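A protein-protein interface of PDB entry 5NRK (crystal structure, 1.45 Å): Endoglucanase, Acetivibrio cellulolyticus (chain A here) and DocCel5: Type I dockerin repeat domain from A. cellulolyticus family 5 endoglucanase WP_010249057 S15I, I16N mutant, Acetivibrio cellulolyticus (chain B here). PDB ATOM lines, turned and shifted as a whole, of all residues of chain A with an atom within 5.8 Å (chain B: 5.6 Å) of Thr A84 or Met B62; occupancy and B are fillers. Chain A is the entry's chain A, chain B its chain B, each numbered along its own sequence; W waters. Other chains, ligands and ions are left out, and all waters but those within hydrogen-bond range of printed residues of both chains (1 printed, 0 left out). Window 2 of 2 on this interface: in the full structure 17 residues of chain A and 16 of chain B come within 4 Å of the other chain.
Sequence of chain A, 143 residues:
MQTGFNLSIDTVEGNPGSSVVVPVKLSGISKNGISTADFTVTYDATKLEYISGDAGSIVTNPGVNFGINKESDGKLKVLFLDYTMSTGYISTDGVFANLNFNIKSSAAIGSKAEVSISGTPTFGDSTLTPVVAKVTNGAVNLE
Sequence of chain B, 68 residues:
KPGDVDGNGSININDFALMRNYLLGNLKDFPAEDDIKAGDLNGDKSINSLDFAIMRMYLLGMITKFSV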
ATOM      1  N   ASN A  65     -15.346 -11.924  12.842  1.00  0.00           N
ATOM      2  CA  ASN A  65     -13.926 -12.062  13.169  1.00  0.00           C
ATOM      3  C   ASN A  65     -13.024 -10.977  12.601  1.00  0.00           C
ATOM      4  O   ASN A  65     -11.932 -10.753  13.124  1.00  0.00           O
ATOM      5  CB  ASN A  65     -13.405 -13.397  12.664  1.00  0.00           C
ATOM      6  CG  ASN A  65     -13.948 -14.578  13.426  1.00  0.00           C
ATOM      7  OD1 ASN A  65     -14.620 -14.431  14.452  1.00  0.00           O
ATOM      8  ND2 ASN A  65     -13.629 -15.772  12.947  1.00  0.00           N
ATOM      9  N   LEU A  81      -9.698 -11.739  14.735  1.00  0.00           N
ATOM     10  CA  LEU A  81      -9.724 -12.655  15.885  1.00  0.00           C
ATOM     11  C   LEU A  81     -10.714 -13.761  15.598  1.00  0.00           C
ATOM     12  O   LEU A  81     -11.839 -13.493  15.204  1.00  0.00           O
ATOM     13  CB  LEU A  81     -10.163 -11.928  17.162  1.00  0.00           C
ATOM     14  CG  LEU A  81     -10.399 -12.801  18.395  1.00  0.00           C
ATOM     15  CD1 LEU A  81      -9.119 -13.512  18.818  1.00  0.00           C
ATOM     16  CD2 LEU A  81     -10.990 -12.000  19.552  1.00  0.00           C
ATOM     17  N   ASP A  82     -10.304 -15.000  15.841  1.00  0.00           N
ATOM     18  CA  ASP A  82     -11.268 -16.097  15.911  1.00  0.00           C
ATOM     19  C   ASP A  82     -12.090 -15.909  17.184  1.00  0.00           C
ATOM     20  O   ASP A  82     -11.620 -16.247  18.267  1.00  0.00           O
ATOM     21  CB  ASP A  82     -10.540 -17.433  15.959  1.00  0.00           C
ATOM     22  CG  ASP A  82     -11.469 -18.600  16.235  1.00  0.00           C
ATOM     23  OD1 ASP A  82     -12.703 -18.427  16.171  1.00  0.00           O
ATOM     24  OD2 ASP A  82     -10.961 -19.722  16.500  1.00  0.00           O
ATOM     25  N   TYR A  83     -13.306 -15.375  17.074  1.00  0.00           N
ATOM     26  CA  TYR A  83     -14.100 -15.104  18.277  1.00  0.00           C
ATOM     27  C   TYR A  83     -14.456 -16.367  19.054  1.00  0.00           C
ATOM     28  O   TYR A  83     -14.827 -16.266  20.224  1.00  0.00           O
ATOM     29  CB  TYR A  83     -15.373 -14.307  17.954  1.00  0.00           C
ATOM     30  CG  TYR A  83     -15.220 -12.788  17.925  1.00  0.00           C
ATOM     31  CD1 TYR A  83     -14.129 -12.167  17.321  1.00  0.00           C
ATOM     32  CD2 TYR A  83     -16.198 -11.981  18.473  1.00  0.00           C
ATOM     33  CE1 TYR A  83     -14.018 -10.786  17.257  1.00  0.00           C
ATOM     34  CE2 TYR A  83     -16.094 -10.593  18.414  1.00  0.00           C
ATOM     35  CZ  TYR A  83     -15.020 -10.006  17.798  1.00  0.00           C
ATOM     36  OH  TYR A  83     -14.899  -8.635  17.731  1.00  0.00           O
ATOM     37  N   THR A  84     -14.357 -17.551  18.438  1.00  0.00           N
ATOM     38  CA  THR A  84     -14.543 -18.813  19.189  1.00  0.00           C
ATOM     39  C   THR A  84     -13.309 -19.233  19.976  1.00  0.00           C
ATOM     40  O   THR A  84     -13.399 -20.084  20.876  1.00  0.00           O
ATOM     41  CB  THR A  84     -14.941 -20.003  18.292  1.00  0.00           C
ATOM     42  OG1 THR A  84     -13.814 -20.473  17.529  1.00  0.00           O
ATOM     43  CG2 THR A  84     -16.080 -19.670  17.383  1.00  0.00           C
ATOM     44  N   MET A  85     -12.148 -18.705  19.595  1.00  0.00           N
ATOM     45  CA  MET A  85     -10.846 -19.172  20.088  1.00  0.00           C
ATOM     46  C   MET A  85     -10.780 -20.696  20.192  1.00  0.00           C
ATOM     47  O   MET A  85     -10.274 -21.263  21.170  1.00  0.00           O
ATOM     48  CB  MET A  85     -10.426 -18.450  21.387  1.00  0.00           C
ATOM     49  CG  MET A  85      -9.734 -17.100  21.094  1.00  0.00           C
ATOM     50  SD  MET A  85      -8.393 -17.123  19.890  1.00  0.00           S
ATOM     51  CE  MET A  85      -7.367 -18.433  20.547  1.00  0.00           C
ATOM     52  N   SER A  86     -11.240 -21.337  19.149  1.00  0.00           N
ATOM     53  CA  SER A  86     -11.282 -22.785  19.071  1.00  0.00           C
ATOM     54  C   SER A  86     -11.299 -23.346  17.638  1.00  0.00           C
ATOM     55  O   SER A  86     -10.486 -24.071  17.304  1.00  0.00           O
ATOM     56  CB  SER A  86     -12.552 -23.267  19.799  1.00  0.00           C
ATOM     57  OG  SER A  86     -12.626 -24.674  19.783  1.00  0.00           O
ATOM     58  N   THR A  87     -12.303 -23.025  16.869  1.00  0.00           N
ATOM     59  CA  THR A  87     -12.600 -23.694  15.615  1.00  0.00           C
ATOM     60  C   THR A  87     -12.413 -22.803  14.393  1.00  0.00           C
ATOM     61  O   THR A  87     -12.735 -23.199  13.270  1.00  0.00           O
ATOM     62  CB  THR A  87     -14.052 -24.201  15.623  1.00  0.00           C
ATOM     63  OG1 THR A  87     -14.936 -23.113  15.928  1.00  0.00           O
ATOM     64  CG2 THR A  87     -14.243 -25.298  16.655  1.00  0.00           C
ATOM     65  N   GLY A  88     -11.896 -21.601  14.596  1.00  0.00           N
ATOM     66  CA  GLY A  88     -11.939 -20.605  13.563  1.00  0.00           C
ATOM     67  C   GLY A  88     -10.631 -19.960  13.225  1.00  0.00           C
ATOM     68  O   GLY A  88     -10.575 -18.844  12.716  1.00  0.00           O
ATOM     69  N   ARG B  56     -11.166 -12.290  25.119  1.00  0.00           N
ATOM     70  CA  ARG B  56     -12.270 -13.068  24.581  1.00  0.00           C
ATOM     71  C   ARG B  56     -12.374 -14.408  25.308  1.00  0.00           C
ATOM     72  O   ARG B  56     -13.471 -14.825  25.695  1.00  0.00           O
ATOM     73  CB  ARG B  56     -12.105 -13.280  23.076  1.00  0.00           C
ATOM     74  CG  ARG B  56     -13.241 -14.051  22.442  1.00  0.00           C
ATOM     75  CD  ARG B  56     -14.575 -13.352  22.530  1.00  0.00           C
ATOM     76  NE  ARG B  56     -15.587 -14.087  21.793  1.00  0.00           N
ATOM     77  CZ  ARG B  56     -16.867 -13.740  21.715  1.00  0.00           C
ATOM     78  NH1 ARG B  56     -17.317 -12.656  22.337  1.00  0.00           N
ATOM     79  NH2 ARG B  56     -17.704 -14.493  21.019  1.00  0.00           N
ATOM     80  N   MET B  57     -11.262 -15.109  25.493  1.00  0.00           N
ATOM     81  CA  MET B  57     -11.295 -16.392  26.197  1.00  0.00           C
ATOM     82  C   MET B  57     -11.850 -16.237  27.607  1.00  0.00           C
ATOM     83  O   MET B  57     -12.624 -17.054  28.079  1.00  0.00           O
ATOM     84  CB  MET B  57      -9.895 -17.005  26.245  1.00  0.00           C
ATOM     85  CG  MET B  57      -9.385 -17.477  24.892  1.00  0.00           C
ATOM     86  SD  MET B  57      -7.803 -18.344  25.020  1.00  0.00           S
ATOM     87  CE  MET B  57      -8.405 -19.938  25.527  1.00  0.00           C
ATOM     88  N   TYR B  58     -11.450 -15.175  28.288  1.00  0.00           N
ATOM     89  CA  TYR B  58     -11.975 -14.907  29.629  1.00  0.00           C
ATOM     90  C   TYR B  58     -13.491 -14.655  29.622  1.00  0.00           C
ATOM     91  O   TYR B  58     -14.220 -15.260  30.422  1.00  0.00           O
ATOM     92  CB  TYR B  58     -11.221 -13.726  30.236  1.00  0.00           C
ATOM     93  CG  TYR B  58     -11.747 -13.283  31.586  1.00  0.00           C
ATOM     94  CD1 TYR B  58     -11.352 -13.899  32.761  1.00  0.00           C
ATOM     95  CD2 TYR B  58     -12.658 -12.234  31.666  1.00  0.00           C
ATOM     96  CE1 TYR B  58     -11.843 -13.461  33.981  1.00  0.00           C
ATOM     97  CE2 TYR B  58     -13.153 -11.792  32.865  1.00  0.00           C
ATOM     98  CZ  TYR B  58     -12.741 -12.407  34.019  1.00  0.00           C
ATOM     99  OH  TYR B  58     -13.225 -11.982  35.250  1.00  0.00           O
ATOM    100  N   LEU B  60     -15.617 -15.666  27.452  1.00  0.00           N
ATOM    101  CA  LEU B  60     -16.303 -16.899  27.070  1.00  0.00           C
ATOM    102  C   LEU B  60     -16.275 -17.944  28.179  1.00  0.00           C
ATOM    103  O   LEU B  60     -16.913 -18.993  28.055  1.00  0.00           O
ATOM    104  CB  LEU B  60     -15.661 -17.507  25.827  1.00  0.00           C
ATOM    105  CG  LEU B  60     -15.894 -16.788  24.499  1.00  0.00           C
ATOM    106  CD1 LEU B  60     -15.033 -17.423  23.427  1.00  0.00           C
ATOM    107  CD2 LEU B  60     -17.356 -16.819  24.106  1.00  0.00           C
ATOM    108  N   GLY B  61     -15.522 -17.691  29.243  1.00  0.00           N
ATOM    109  CA  GLY B  61     -15.370 -18.667  30.315  1.00  0.00           C
ATOM    110  C   GLY B  61     -14.383 -19.794  30.018  1.00  0.00           C
ATOM    111  O   GLY B  61     -14.371 -20.812  30.719  1.00  0.00           O
ATOM    112  N   MET B  62     -13.523 -19.596  29.030  1.00  0.00           N
ATOM    113  CA  MET B  62     -12.556 -20.602  28.621  1.00  0.00           C
ATOM    114  C   MET B  62     -11.313 -20.592  29.510  1.00  0.00           C
ATOM    115  O   MET B  62     -10.599 -21.587  29.580  1.00  0.00           O
ATOM    116  CB  MET B  62     -12.177 -20.388  27.159  1.00  0.00           C
ATOM    117  CG  MET B  62     -13.358 -20.552  26.199  1.00  0.00           C
ATOM    118  SD  MET B  62     -13.139 -20.028  24.490  1.00  0.00           S
ATOM    119  CE  MET B  62     -12.233 -21.443  23.878  1.00  0.00           C
ATOM    120  N   ILE B  63     -11.059 -19.447  30.148  1.00  0.00           N
ATOM    121  CA  ILE B  63     -10.005 -19.289  31.160  1.00  0.00           C
ATOM    122  C   ILE B  63     -10.621 -18.548  32.323  1.00  0.00           C
ATOM    123  O   ILE B  63     -11.691 -17.923  32.194  1.00  0.00           O
ATOM    124  CB  ILE B  63      -8.764 -18.526  30.648  1.00  0.00           C
ATOM    125  CG1 ILE B  63      -9.098 -17.072  30.259  1.00  0.00           C
ATOM    126  CG2 ILE B  63      -8.135 -19.292  29.503  1.00  0.00           C
ATOM    127  CD1 ILE B  63      -7.888 -16.254  29.816  1.00  0.00           C
ATOM    128  N   THR B  64      -9.945 -18.631  33.462  1.00  0.00           N
ATOM    129  CA  THR B  64     -10.438 -18.089  34.710  1.00  0.00           C
ATOM    130  C   THR B  64      -9.674 -16.834  35.143  1.00  0.00           C
ATOM    131  O   THR B  64     -10.229 -15.950  35.785  1.00  0.00           O
ATOM    132  CB  THR B  64     -10.320 -19.180  35.796  1.00  0.00           C
ATOM    133  OG1 THR B  64     -11.179 -20.286  35.460  1.00  0.00           O
ATOM    134  CG2 THR B  64     -10.689 -18.665  37.159  1.00  0.00           C
HETATM  135  O   HOH W   1     -18.093 -17.075  19.806  1.00  0.00           O
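The backbone carbonyl oxygen (O) of Thr A84 sits close to the side-chain sulfur (SD) of Met B62 (3.6 Å). O of Tyr A83 sits at hydrogen-bond distance from NE of Arg B56, at 2.8 Å.
N of Met B62 is in hydrogen-bond range of O of Met B57, at 2.9 Å. The backbone NH (N) of Tyr A83 lies within hydrogen-bond range of the side-chain amide oxygen (OD1) of Asn A65 (3.1 Å). N of Met A85 sits close to OD2 of Asp A82, 3.5 Å away. OD1 of Asp A82 sits at hydrogen-bond distance from OG1 of Thr A84. OG1 of Thr A84 lies close to N of Ser A86, at 3.2 Å. N of Leu A81 lies within hydrogen-bond range of O of Asn A65 (2.9 Å).
Among the printed residues, pairs that only touch across the chains: Met A85 with Met B62, Tyr A83 with Leu B60, Met A85 with Met B57 and Leu A81 with Arg B56.
Printed residues of chain B within 4 Å of Leu A81: Arg B56 (3.9 Å). Printed residues of chain B within 4 Å of Tyr A83: Arg B56 and Leu B60. Printed residues of chain B within 4 Å of Thr A84: Met B62 (3.5 Å). Of the printed residues of chain B, Met A85 touches Met B57 (3.8 Å) and Met B62 (3.3 Å). Printed residues of chain A within 4 Å of Arg B56: Leu A81 (3.9 Å) and Tyr A83 (2.8 Å). Gly B61 touches none of the printed residues of chain A. The nearest printed residue of chain A that does not touch Met B62 is Ser A86 (4.5 Å). The nearest printed residue of chain B that does not touch Met A85 is Arg B56 (4.8 Å).
Hydrophobic or aromatic side chains of chain A within 4 Å of the printed part of chain B: Leu A81, Tyr A83 and Met A85. Of the 8 printed residues of chain B, 4 touch a printed residue of chain A. Hydrophobic or aromatic side chains of chain B that line the printed part of chain A: Met B57, Leu B60 and Met B62. Among the printed residues, 6 pairs touch across the chains. Among the printed residues, no Asp or Glu carboxylate lies within 4 Å of a Lys or Arg side-chain nitrogen of the other chain.
Water W1 bridges the guanidinium group of Arg B56 (2.9 Å) and the backbone carbonyl oxygen of Tyr A83 (3.4 Å).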
